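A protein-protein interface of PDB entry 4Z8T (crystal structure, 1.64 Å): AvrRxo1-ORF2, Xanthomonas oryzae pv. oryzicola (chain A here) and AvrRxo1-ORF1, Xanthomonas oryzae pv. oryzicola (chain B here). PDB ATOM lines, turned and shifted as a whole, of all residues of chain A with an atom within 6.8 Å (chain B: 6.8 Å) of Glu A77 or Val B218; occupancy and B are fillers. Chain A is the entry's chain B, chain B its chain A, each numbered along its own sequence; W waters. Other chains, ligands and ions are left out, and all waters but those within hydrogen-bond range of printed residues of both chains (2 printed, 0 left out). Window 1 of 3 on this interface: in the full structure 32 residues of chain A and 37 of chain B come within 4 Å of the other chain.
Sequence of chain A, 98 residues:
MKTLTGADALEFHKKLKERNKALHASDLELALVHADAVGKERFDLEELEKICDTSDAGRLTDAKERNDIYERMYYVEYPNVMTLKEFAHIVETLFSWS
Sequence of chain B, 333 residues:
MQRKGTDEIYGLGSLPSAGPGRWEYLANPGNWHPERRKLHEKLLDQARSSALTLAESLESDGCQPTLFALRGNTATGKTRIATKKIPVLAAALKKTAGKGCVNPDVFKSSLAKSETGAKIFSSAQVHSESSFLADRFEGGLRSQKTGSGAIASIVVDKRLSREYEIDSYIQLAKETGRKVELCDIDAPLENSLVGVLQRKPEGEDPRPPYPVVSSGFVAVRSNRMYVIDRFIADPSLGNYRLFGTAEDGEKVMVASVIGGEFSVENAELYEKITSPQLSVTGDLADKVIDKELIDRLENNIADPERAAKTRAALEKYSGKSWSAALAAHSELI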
ATOM      1  N   ALA A  31      16.666  32.631 -23.791  1.00  0.00           N
ATOM      2  CA  ALA A  31      16.033  32.657 -22.488  1.00  0.00           C
ATOM      3  C   ALA A  31      16.552  33.828 -21.657  1.00  0.00           C
ATOM      4  O   ALA A  31      15.785  34.438 -20.916  1.00  0.00           O
ATOM      5  CB  ALA A  31      16.259  31.349 -21.765  1.00  0.00           C
ATOM      6  N   LYS A  40      13.348  38.967 -14.502  1.00  0.00           N
ATOM      7  CA  LYS A  40      13.630  37.747 -13.753  1.00  0.00           C
ATOM      8  C   LYS A  40      14.913  37.919 -12.941  1.00  0.00           C
ATOM      9  O   LYS A  40      15.888  38.489 -13.429  1.00  0.00           O
ATOM     10  CB  LYS A  40      13.757  36.573 -14.734  1.00  0.00           C
ATOM     11  CG  LYS A  40      14.137  35.222 -14.131  1.00  0.00           C
ATOM     12  CD  LYS A  40      13.830  34.124 -15.149  1.00  0.00           C
ATOM     13  CE  LYS A  40      14.355  32.775 -14.708  1.00  0.00           C
ATOM     14  NZ  LYS A  40      13.385  31.707 -15.078  1.00  0.00           N
ATOM     15  N   ILE A  69      24.380  23.245 -14.807  1.00  0.00           N
ATOM     16  CA  ILE A  69      23.129  22.504 -14.661  1.00  0.00           C
ATOM     17  C   ILE A  69      21.995  23.408 -14.172  1.00  0.00           C
ATOM     18  O   ILE A  69      20.907  23.434 -14.759  1.00  0.00           O
ATOM     19  CB  ILE A  69      23.283  21.303 -13.691  1.00  0.00           C
ATOM     20  CG1 ILE A  69      24.098  20.182 -14.342  1.00  0.00           C
ATOM     21  CG2 ILE A  69      21.929  20.764 -13.281  1.00  0.00           C
ATOM     22  CD1 ILE A  69      24.582  19.137 -13.355  1.00  0.00           C
ATOM     23  N   GLU A  71      21.899  26.898 -13.637  1.00  0.00           N
ATOM     24  CA  GLU A  71      21.672  28.155 -14.343  1.00  0.00           C
ATOM     25  C   GLU A  71      20.807  27.875 -15.564  1.00  0.00           C
ATOM     26  O   GLU A  71      19.805  28.554 -15.802  1.00  0.00           O
ATOM     27  CB  GLU A  71      22.993  28.815 -14.760  1.00  0.00           C
ATOM     28  CG  GLU A  71      22.888  29.607 -16.065  1.00  0.00           C
ATOM     29  CD  GLU A  71      23.702  30.882 -16.063  1.00  0.00           C
ATOM     30  OE1 GLU A  71      24.172  31.291 -14.975  1.00  0.00           O
ATOM     31  OE2 GLU A  71      23.857  31.484 -17.151  1.00  0.00           O
ATOM     32  N   ARG A  72      21.187  26.856 -16.324  1.00  0.00           N
ATOM     33  CA  ARG A  72      20.443  26.497 -17.526  1.00  0.00           C
ATOM     34  C   ARG A  72      19.019  26.055 -17.194  1.00  0.00           C
ATOM     35  O   ARG A  72      18.069  26.466 -17.853  1.00  0.00           O
ATOM     36  CB  ARG A  72      21.183  25.414 -18.309  1.00  0.00           C
ATOM     37  CG  ARG A  72      20.400  24.860 -19.470  1.00  0.00           C
ATOM     38  CD  ARG A  72      21.233  23.890 -20.287  1.00  0.00           C
ATOM     39  NE  ARG A  72      22.313  24.585 -20.971  1.00  0.00           N
ATOM     40  CZ  ARG A  72      22.145  25.295 -22.085  1.00  0.00           C
ATOM     41  NH1 ARG A  72      23.184  25.897 -22.638  1.00  0.00           N
ATOM     42  NH2 ARG A  72      20.936  25.399 -22.645  1.00  0.00           N
ATOM     43  N   MET A  73      18.861  25.229 -16.166  1.00  0.00           N
ATOM     44  CA  MET A  73      17.519  24.821 -15.758  1.00  0.00           C
ATOM     45  C   MET A  73      16.663  26.031 -15.389  1.00  0.00           C
ATOM     46  O   MET A  73      15.522  26.162 -15.815  1.00  0.00           O
ATOM     47  CB  MET A  73      17.582  23.830 -14.589  1.00  0.00           C
ATOM     48  CG  MET A  73      16.225  23.388 -14.117  1.00  0.00           C
ATOM     49  SD  MET A  73      16.415  22.224 -12.561  1.00  0.00           S
ATOM     50  CE  MET A  73      17.500  20.879 -13.391  1.00  0.00           C
ATOM     51  N   TYR A  74      17.244  26.940 -14.616  1.00  0.00           N
ATOM     52  CA  TYR A  74      16.540  28.124 -14.156  1.00  0.00           C
ATOM     53  C   TYR A  74      16.005  28.948 -15.329  1.00  0.00           C
ATOM     54  O   TYR A  74      14.833  29.327 -15.356  1.00  0.00           O
ATOM     55  CB  TYR A  74      17.514  28.954 -13.316  1.00  0.00           C
ATOM     56  CG  TYR A  74      16.984  30.266 -12.771  1.00  0.00           C
ATOM     57  CD1 TYR A  74      15.952  30.294 -11.848  1.00  0.00           C
ATOM     58  CD2 TYR A  74      17.547  31.472 -13.164  1.00  0.00           C
ATOM     59  CE1 TYR A  74      15.486  31.493 -11.334  1.00  0.00           C
ATOM     60  CE2 TYR A  74      17.090  32.671 -12.655  1.00  0.00           C
ATOM     61  CZ  TYR A  74      16.061  32.675 -11.746  1.00  0.00           C
ATOM     62  OH  TYR A  74      15.601  33.866 -11.240  1.00  0.00           O
ATOM     63  N   TYR A  75      16.867  29.197 -16.306  1.00  0.00           N
ATOM     64  CA  TYR A  75      16.512  30.079 -17.411  1.00  0.00           C
ATOM     65  C   TYR A  75      15.739  29.389 -18.525  1.00  0.00           C
ATOM     66  O   TYR A  75      14.804  29.967 -19.064  1.00  0.00           O
ATOM     67  CB  TYR A  75      17.753  30.734 -18.003  1.00  0.00           C
ATOM     68  CG  TYR A  75      18.282  31.867 -17.150  1.00  0.00           C
ATOM     69  CD1 TYR A  75      17.485  32.966 -16.861  1.00  0.00           C
ATOM     70  CD2 TYR A  75      19.572  31.833 -16.644  1.00  0.00           C
ATOM     71  CE1 TYR A  75      17.964  34.010 -16.081  1.00  0.00           C
ATOM     72  CE2 TYR A  75      20.065  32.876 -15.861  1.00  0.00           C
ATOM     73  CZ  TYR A  75      19.247  33.956 -15.588  1.00  0.00           C
ATOM     74  OH  TYR A  75      19.708  34.996 -14.812  1.00  0.00           O
ATOM     75  N   VAL A  76      16.145  28.171 -18.875  1.00  0.00           N
ATOM     76  CA  VAL A  76      15.575  27.501 -20.047  1.00  0.00           C
ATOM     77  C   VAL A  76      14.337  26.688 -19.707  1.00  0.00           C
ATOM     78  O   VAL A  76      13.338  26.734 -20.426  1.00  0.00           O
ATOM     79  CB  VAL A  76      16.608  26.611 -20.735  1.00  0.00           C
ATOM     80  CG1 VAL A  76      15.996  25.914 -21.938  1.00  0.00           C
ATOM     81  CG2 VAL A  76      17.788  27.441 -21.177  1.00  0.00           C
ATOM     82  N   GLU A  77      14.386  25.954 -18.601  1.00  0.00           N
ATOM     83  CA  GLU A  77      13.272  25.068 -18.267  1.00  0.00           C
ATOM     84  C   GLU A  77      12.162  25.725 -17.470  1.00  0.00           C
ATOM     85  O   GLU A  77      11.023  25.274 -17.512  1.00  0.00           O
ATOM     86  CB  GLU A  77      13.777  23.851 -17.505  1.00  0.00           C
ATOM     87  CG  GLU A  77      14.620  22.913 -18.310  1.00  0.00           C
ATOM     88  CD  GLU A  77      14.981  21.690 -17.498  1.00  0.00           C
ATOM     89  OE1 GLU A  77      16.190  21.412 -17.333  1.00  0.00           O
ATOM     90  OE2 GLU A  77      14.045  21.014 -17.005  1.00  0.00           O
ATOM     91  N   TYR A  78      12.485  26.783 -16.730  1.00  0.00           N
ATOM     92  CA  TYR A  78      11.473  27.437 -15.900  1.00  0.00           C
ATOM     93  C   TYR A  78      11.426  28.935 -16.165  1.00  0.00           C
ATOM     94  O   TYR A  78      11.725  29.742 -15.272  1.00  0.00           O
ATOM     95  CB  TYR A  78      11.706  27.123 -14.412  1.00  0.00           C
ATOM     96  CG  TYR A  78      11.605  25.636 -14.132  1.00  0.00           C
ATOM     97  CD1 TYR A  78      10.387  25.049 -13.819  1.00  0.00           C
ATOM     98  CD2 TYR A  78      12.722  24.818 -14.227  1.00  0.00           C
ATOM     99  CE1 TYR A  78      10.286  23.692 -13.589  1.00  0.00           C
ATOM    100  CE2 TYR A  78      12.634  23.454 -14.000  1.00  0.00           C
ATOM    101  CZ  TYR A  78      11.408  22.901 -13.680  1.00  0.00           C
ATOM    102  OH  TYR A  78      11.311  21.551 -13.461  1.00  0.00           O
ATOM    103  N   PRO A  79      11.052  29.310 -17.403  1.00  0.00           N
ATOM    104  CA  PRO A  79      11.090  30.719 -17.810  1.00  0.00           C
ATOM    105  C   PRO A  79      10.112  31.594 -17.035  1.00  0.00           C
ATOM    106  O   PRO A  79      10.370  32.792 -16.914  1.00  0.00           O
ATOM    107  CB  PRO A  79      10.696  30.666 -19.294  1.00  0.00           C
ATOM    108  CG  PRO A  79       9.894  29.425 -19.437  1.00  0.00           C
ATOM    109  CD  PRO A  79      10.518  28.446 -18.476  1.00  0.00           C
ATOM    110  N   ASN A  80       9.023  31.020 -16.531  1.00  0.00           N
ATOM    111  CA  ASN A  80       8.022  31.796 -15.801  1.00  0.00           C
ATOM    112  C   ASN A  80       8.328  31.935 -14.307  1.00  0.00           C
ATOM    113  O   ASN A  80       7.623  32.642 -13.583  1.00  0.00           O
ATOM    114  CB  ASN A  80       6.623  31.209 -16.005  1.00  0.00           C
ATOM    115  CG  ASN A  80       6.205  31.191 -17.469  1.00  0.00           C
ATOM    116  OD1 ASN A  80       6.581  32.067 -18.252  1.00  0.00           O
ATOM    117  ND2 ASN A  80       5.428  30.180 -17.845  1.00  0.00           N
ATOM    118  N   VAL A  81       9.371  31.245 -13.853  1.00  0.00           N
ATOM    119  CA  VAL A  81       9.866  31.387 -12.485  1.00  0.00           C
ATOM    120  C   VAL A  81      10.731  32.642 -12.399  1.00  0.00           C
ATOM    121  O   VAL A  81      11.713  32.773 -13.126  1.00  0.00           O
ATOM    122  CB  VAL A  81      10.682  30.148 -12.062  1.00  0.00           C
ATOM    123  CG1 VAL A  81      11.414  30.397 -10.750  1.00  0.00           C
ATOM    124  CG2 VAL A  81       9.771  28.931 -11.956  1.00  0.00           C
ATOM    125  N   PHE A  87      12.601  28.990  -7.415  1.00  0.00           N
ATOM    126  CA  PHE A  87      13.364  27.923  -8.048  1.00  0.00           C
ATOM    127  C   PHE A  87      13.842  26.921  -7.009  1.00  0.00           C
ATOM    128  O   PHE A  87      13.912  25.725  -7.279  1.00  0.00           O
ATOM    129  CB  PHE A  87      14.553  28.517  -8.805  1.00  0.00           C
ATOM    130  CG  PHE A  87      15.312  27.518  -9.633  1.00  0.00           C
ATOM    131  CD1 PHE A  87      14.675  26.794 -10.628  1.00  0.00           C
ATOM    132  CD2 PHE A  87      16.663  27.320  -9.432  1.00  0.00           C
ATOM    133  CE1 PHE A  87      15.376  25.887 -11.390  1.00  0.00           C
ATOM    134  CE2 PHE A  87      17.372  26.416 -10.192  1.00  0.00           C
ATOM    135  CZ  PHE A  87      16.725  25.696 -11.178  1.00  0.00           C
ATOM    136  N   LEU A  94      12.788  18.163  -6.988  1.00  0.00           N
ATOM    137  CA  LEU A  94      13.571  17.272  -7.837  1.00  0.00           C
ATOM    138  C   LEU A  94      14.375  16.247  -7.053  1.00  0.00           C
ATOM    139  O   LEU A  94      14.533  15.111  -7.491  1.00  0.00           O
ATOM    140  CB  LEU A  94      14.509  18.056  -8.751  1.00  0.00           C
ATOM    141  CG  LEU A  94      13.861  18.926  -9.821  1.00  0.00           C
ATOM    142  CD1 LEU A  94      14.945  19.506 -10.711  1.00  0.00           C
ATOM    143  CD2 LEU A  94      12.880  18.122 -10.645  1.00  0.00           C
ATOM    144  N   ASN B  73      14.415   8.128 -18.792  1.00  0.00           N
ATOM    145  CA  ASN B  73      13.491   8.867 -17.950  1.00  0.00           C
ATOM    146  C   ASN B  73      12.402   7.974 -17.347  1.00  0.00           C
ATOM    147  O   ASN B  73      12.204   6.828 -17.742  1.00  0.00           O
ATOM    148  CB  ASN B  73      12.843   9.988 -18.774  1.00  0.00           C
ATOM    149  CG  ASN B  73      12.211  11.062 -17.915  1.00  0.00           C
ATOM    150  OD1 ASN B  73      12.625  11.292 -16.772  1.00  0.00           O
ATOM    151  ND2 ASN B  73      11.196  11.740 -18.471  1.00  0.00           N
ATOM    152  N   SER B 161      20.873  10.401 -16.075  1.00  0.00           N
ATOM    153  CA  SER B 161      20.765  11.415 -17.115  1.00  0.00           C
ATOM    154  C   SER B 161      22.096  12.131 -17.347  1.00  0.00           C
ATOM    155  O   SER B 161      22.557  12.224 -18.490  1.00  0.00           O
ATOM    156  CB  SER B 161      19.604  12.388 -16.851  1.00  0.00           C
ATOM    157  OG  SER B 161      19.722  13.093 -15.627  1.00  0.00           O
ATOM    158  N   ARG B 162      22.743  12.567 -16.267  1.00  0.00           N
ATOM    159  CA  ARG B 162      23.814  13.556 -16.399  1.00  0.00           C
ATOM    160  C   ARG B 162      25.232  13.018 -16.519  1.00  0.00           C
ATOM    161  O   ARG B 162      25.520  11.884 -16.129  1.00  0.00           O
ATOM    162  CB  ARG B 162      23.719  14.575 -15.270  1.00  0.00           C
ATOM    163  CG  ARG B 162      22.341  15.191 -15.196  1.00  0.00           C
ATOM    164  CD  ARG B 162      22.325  16.468 -14.400  1.00  0.00           C
ATOM    165  NE  ARG B 162      20.949  16.862 -14.136  1.00  0.00           N
ATOM    166  CZ  ARG B 162      20.236  17.656 -14.924  1.00  0.00           C
ATOM    167  NH1 ARG B 162      18.983  17.947 -14.599  1.00  0.00           N
ATOM    168  NH2 ARG B 162      20.773  18.160 -16.026  1.00  0.00           N
ATOM    169  N   LEU B 189       7.811  12.863 -23.898  1.00  0.00           N
ATOM    170  CA  LEU B 189       7.467  13.306 -22.553  1.00  0.00           C
ATOM    171  C   LEU B 189       6.038  12.955 -22.191  1.00  0.00           C
ATOM    172  O   LEU B 189       5.775  12.510 -21.082  1.00  0.00           O
ATOM    173  CB  LEU B 189       7.695  14.806 -22.418  1.00  0.00           C
ATOM    174  CG  LEU B 189       7.293  15.474 -21.100  1.00  0.00           C
ATOM    175  CD1 LEU B 189       7.931  14.797 -19.900  1.00  0.00           C
ATOM    176  CD2 LEU B 189       7.710  16.941 -21.147  1.00  0.00           C
ATOM    177  N   PRO B 211       7.422  18.279 -12.460  1.00  0.00           N
ATOM    178  CA  PRO B 211       8.780  18.782 -12.694  1.00  0.00           C
ATOM    179  C   PRO B 211       9.849  17.682 -12.743  1.00  0.00           C
ATOM    180  O   PRO B 211      10.845  17.817 -13.465  1.00  0.00           O
ATOM    181  CB  PRO B 211       9.028  19.699 -11.490  1.00  0.00           C
ATOM    182  CG  PRO B 211       7.660  20.142 -11.079  1.00  0.00           C
ATOM    183  CD  PRO B 211       6.803  18.918 -11.280  1.00  0.00           C
ATOM    184  N   VAL B 213       9.457  14.619 -13.960  1.00  0.00           N
ATOM    185  CA  VAL B 213       9.376  13.941 -15.251  1.00  0.00           C
ATOM    186  C   VAL B 213       9.875  14.836 -16.388  1.00  0.00           C
ATOM    187  O   VAL B 213      10.600  14.386 -17.287  1.00  0.00           O
ATOM    188  CB  VAL B 213       7.933  13.460 -15.504  1.00  0.00           C
ATOM    189  CG1 VAL B 213       7.860  12.635 -16.790  1.00  0.00           C
ATOM    190  CG2 VAL B 213       7.459  12.627 -14.311  1.00  0.00           C
ATOM    191  N   SER B 214       9.530  16.117 -16.342  1.00  0.00           N
ATOM    192  CA  SER B 214       9.974  17.047 -17.386  1.00  0.00           C
ATOM    193  C   SER B 214      11.463  17.345 -17.309  1.00  0.00           C
ATOM    194  O   SER B 214      12.170  17.279 -18.317  1.00  0.00           O
ATOM    195  CB  SER B 214       9.154  18.339 -17.338  1.00  0.00           C
ATOM    196  OG  SER B 214       9.486  19.168 -18.443  1.00  0.00           O
ATOM    197  N   SER B 215      11.959  17.646 -16.117  1.00  0.00           N
ATOM    198  CA  SER B 215      13.380  17.919 -15.997  1.00  0.00           C
ATOM    199  C   SER B 215      14.195  16.667 -16.283  1.00  0.00           C
ATOM    200  O   SER B 215      15.286  16.738 -16.858  1.00  0.00           O
ATOM    201  CB  SER B 215      13.715  18.502 -14.624  1.00  0.00           C
ATOM    202  OG  SER B 215      13.339  19.872 -14.603  1.00  0.00           O
ATOM    203  N   GLY B 216      13.642  15.507 -15.940  1.00  0.00           N
ATOM    204  CA  GLY B 216      14.298  14.251 -16.270  1.00  0.00           C
ATOM    205  C   GLY B 216      14.392  14.035 -17.770  1.00  0.00           C
ATOM    206  O   GLY B 216      15.398  13.530 -18.273  1.00  0.00           O
ATOM    207  N   PHE B 217      13.326  14.401 -18.475  1.00  0.00           N
ATOM    208  CA  PHE B 217      13.262  14.279 -19.925  1.00  0.00           C
ATOM    209  C   PHE B 217      14.300  15.171 -20.575  1.00  0.00           C
ATOM    210  O   PHE B 217      15.043  14.740 -21.459  1.00  0.00           O
ATOM    211  CB  PHE B 217      11.862  14.684 -20.379  1.00  0.00           C
ATOM    212  CG  PHE B 217      11.693  14.804 -21.866  1.00  0.00           C
ATOM    213  CD1 PHE B 217      11.387  13.695 -22.631  1.00  0.00           C
ATOM    214  CD2 PHE B 217      11.749  16.051 -22.489  1.00  0.00           C
ATOM    215  CE1 PHE B 217      11.199  13.814 -23.993  1.00  0.00           C
ATOM    216  CE2 PHE B 217      11.556  16.167 -23.855  1.00  0.00           C
ATOM    217  CZ  PHE B 217      11.286  15.043 -24.603  1.00  0.00           C
ATOM    218  N   VAL B 218      14.341  16.423 -20.141  1.00  0.00           N
ATOM    219  CA  VAL B 218      15.311  17.358 -20.678  1.00  0.00           C
ATOM    220  C   VAL B 218      16.741  16.863 -20.460  1.00  0.00           C
ATOM    221  O   VAL B 218      17.553  16.841 -21.393  1.00  0.00           O
ATOM    222  CB  VAL B 218      15.133  18.755 -20.066  1.00  0.00           C
ATOM    223  CG1 VAL B 218      16.305  19.646 -20.453  1.00  0.00           C
ATOM    224  CG2 VAL B 218      13.811  19.358 -20.529  1.00  0.00           C
ATOM    225  N   ALA B 219      17.030  16.416 -19.241  1.00  0.00           N
ATOM    226  CA  ALA B 219      18.368  15.952 -18.893  1.00  0.00           C
ATOM    227  C   ALA B 219      18.766  14.707 -19.679  1.00  0.00           C
ATOM    228  O   ALA B 219      19.886  14.616 -20.187  1.00  0.00           O
ATOM    229  CB  ALA B 219      18.461  15.686 -17.426  1.00  0.00           C
ATOM    230  N   VAL B 220      17.859  13.739 -19.776  1.00  0.00           N
ATOM    231  CA  VAL B 220      18.210  12.491 -20.439  1.00  0.00           C
ATOM    232  C   VAL B 220      18.468  12.699 -21.929  1.00  0.00           C
ATOM    233  O   VAL B 220      19.386  12.108 -22.495  1.00  0.00           O
ATOM    234  CB  VAL B 220      17.163  11.366 -20.171  1.00  0.00           C
ATOM    235  CG1 VAL B 220      15.960  11.527 -21.048  1.00  0.00           C
ATOM    236  CG2 VAL B 220      17.802   9.989 -20.367  1.00  0.00           C
ATOM    237  N   ARG B 221      17.696  13.575 -22.559  1.00  0.00           N
ATOM    238  CA  ARG B 221      17.903  13.837 -23.964  1.00  0.00           C
ATOM    239  C   ARG B 221      19.150  14.688 -24.210  1.00  0.00           C
ATOM    240  O   ARG B 221      19.929  14.391 -25.108  1.00  0.00           O
ATOM    241  CB  ARG B 221      16.655  14.477 -24.580  1.00  0.00           C
ATOM    242  CG  ARG B 221      15.534  13.459 -24.731  1.00  0.00           C
ATOM    243  CD  ARG B 221      14.726  13.773 -25.920  1.00  0.00           C
ATOM    244  NE  ARG B 221      13.684  12.776 -26.186  1.00  0.00           N
ATOM    245  CZ  ARG B 221      12.664  13.000 -26.995  1.00  0.00           C
ATOM    246  NH1 ARG B 221      12.561  14.172 -27.616  1.00  0.00           N
ATOM    247  NH2 ARG B 221      11.750  12.057 -27.174  1.00  0.00           N
ATOM    248  N   SER B 222      19.331  15.732 -23.410  1.00  0.00           N
ATOM    249  CA  SER B 222      20.439  16.671 -23.636  1.00  0.00           C
ATOM    250  C   SER B 222      21.813  16.026 -23.483  1.00  0.00           C
ATOM    251  O   SER B 222      22.787  16.454 -24.122  1.00  0.00           O
ATOM    252  CB  SER B 222      20.334  17.880 -22.697  1.00  0.00           C
ATOM    253  OG  SER B 222      19.178  18.644 -23.005  1.00  0.00           O
ATOM    254  N   ASN B 223      21.898  15.007 -22.635  1.00  0.00           N
ATOM    255  CA  ASN B 223      23.170  14.356 -22.356  1.00  0.00           C
ATOM    256  C   ASN B 223      23.350  13.007 -23.026  1.00  0.00           C
ATOM    257  O   ASN B 223      24.342  12.329 -22.797  1.00  0.00           O
ATOM    258  CB  ASN B 223      23.365  14.222 -20.850  1.00  0.00           C
ATOM    259  CG  ASN B 223      23.552  15.557 -20.190  1.00  0.00           C
ATOM    260  OD1 ASN B 223      24.546  16.240 -20.447  1.00  0.00           O
ATOM    261  ND2 ASN B 223      22.609  15.949 -19.343  1.00  0.00           N
ATOM    262  N   SER B 275      17.448  15.662 -28.493  1.00  0.00           N
ATOM    263  CA  SER B 275      17.083  17.060 -28.251  1.00  0.00           C
ATOM    264  C   SER B 275      15.785  17.159 -27.442  1.00  0.00           C
ATOM    265  O   SER B 275      14.855  16.395 -27.659  1.00  0.00           O
ATOM    266  CB  SER B 275      16.920  17.760 -29.609  1.00  0.00           C
ATOM    267  OG  SER B 275      15.944  18.779 -29.561  1.00  0.00           O
ATOM    268  N   PRO B 276      15.704  18.116 -26.508  1.00  0.00           N
ATOM    269  CA  PRO B 276      14.506  18.219 -25.657  1.00  0.00           C
ATOM    270  C   PRO B 276      13.293  18.973 -26.241  1.00  0.00           C
ATOM    271  O   PRO B 276      12.258  19.039 -25.566  1.00  0.00           O
ATOM    272  CB  PRO B 276      15.030  18.960 -24.421  1.00  0.00           C
ATOM    273  CG  PRO B 276      16.164  19.779 -24.937  1.00  0.00           C
ATOM    274  CD  PRO B 276      16.798  18.988 -26.045  1.00  0.00           C
ATOM    275  N   LEU B 278      12.644  22.148 -26.531  1.00  0.00           N
ATOM    276  CA  LEU B 278      12.333  23.378 -25.782  1.00  0.00           C
ATOM    277  C   LEU B 278      12.028  24.619 -26.646  1.00  0.00           C
ATOM    278  O   LEU B 278      12.507  24.731 -27.752  1.00  0.00           O
ATOM    279  CB  LEU B 278      13.474  23.738 -24.795  1.00  0.00           C
ATOM    280  CG  LEU B 278      13.861  22.473 -24.066  1.00  0.00           C
ATOM    281  CD1 LEU B 278      15.052  22.584 -23.113  1.00  0.00           C
ATOM    282  CD2 LEU B 278      12.606  21.964 -23.379  1.00  0.00           C
ATOM    283  N   ASP B 283       3.911  25.551 -22.681  1.00  0.00           N
ATOM    284  CA  ASP B 283       4.245  24.723 -21.528  1.00  0.00           C
ATOM    285  C   ASP B 283       3.301  23.531 -21.413  1.00  0.00           C
ATOM    286  O   ASP B 283       2.120  23.688 -21.102  1.00  0.00           O
ATOM    287  CB  ASP B 283       4.203  25.553 -20.243  1.00  0.00           C
ATOM    288  CG  ASP B 283       4.914  24.874 -19.088  1.00  0.00           C
ATOM    289  OD1 ASP B 283       5.347  23.714 -19.254  1.00  0.00           O
ATOM    290  OD2 ASP B 283       5.041  25.501 -18.015  1.00  0.00           O
HETATM  291  O   HOH W   1      16.939  19.079 -16.540  1.00  0.00           O
HETATM  292  O   HOH W   2      11.375  20.966 -17.697  1.00  0.00           O
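The side-chain hydroxyl of Ser B215 lies within hydrogen-bond range of the side-chain carboxylate of Glu A77 (2.8 Å). The side-chain hydroxyl of Ser B215 is in hydrogen-bond range of the side-chain hydroxyl of Tyr A78 (2.9 Å).
O of Pro B211 lies close to OG of Ser B215. The side-chain hydroxyl (OG) of Ser B222 is in hydrogen-bond range of the backbone carbonyl oxygen (O) of Val B218 (2.9 Å). O of Tyr A78 lies within hydrogen-bond range of NZ of Lys A40 (2.6 Å). O of Met A73 sits at hydrogen-bond distance from N of Tyr A78 (3.2 Å).
Among the printed residues, pairs that only touch across the chains: Ile A69 with Arg B162, Met A73 with Arg B162, Val A76 with Leu B278, Glu A77 with Val B218, Tyr A78 with Pro B211 and Leu A94 with Pro B211.
Printed residues of chain B within 4 Å of Glu A77: Ser B215 (2.8 Å) and Val B218 (3.6 Å). Of the printed residues of chain A, Val B218 touches Glu A77 (3.6 Å). Of the printed residues of chain B, Met A73 touches Arg B162 (3.5 Å). Of the printed residues of chain B, Ile A69 touches Arg B162. Of the printed residues of chain B, Val A76 touches Leu B278 (3.7 Å). Of the printed residues of chain B, Tyr A78 touches Pro B211 (3.5 Å) and Ser B215 (2.9 Å). Tyr A75 touches none of the printed residues of chain B. Ala B219 touches none of the printed residues of chain A. The nearest printed residue of chain A that does not touch Leu B278 is Glu A77 (4.8 Å).
Among the printed residues, 8 pairs touch across the chains. Among the printed residues, no Asp or Glu carboxylate lies within 4 Å of a Lys or Arg side-chain nitrogen of the other chain.
Water W1 lies within hydrogen-bond range of the side-chain carboxylate of Glu A77 (2.6 Å), the backbone carbonyl oxygen of Ser B215 (2.9 Å) and the guanidinium group of Arg B162 (3.0 Å). Water W2 bridges the side-chain hydroxyl of Ser B214 (2.7 Å) and the side-chain carboxylate of Glu A77 (2.8 Å).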
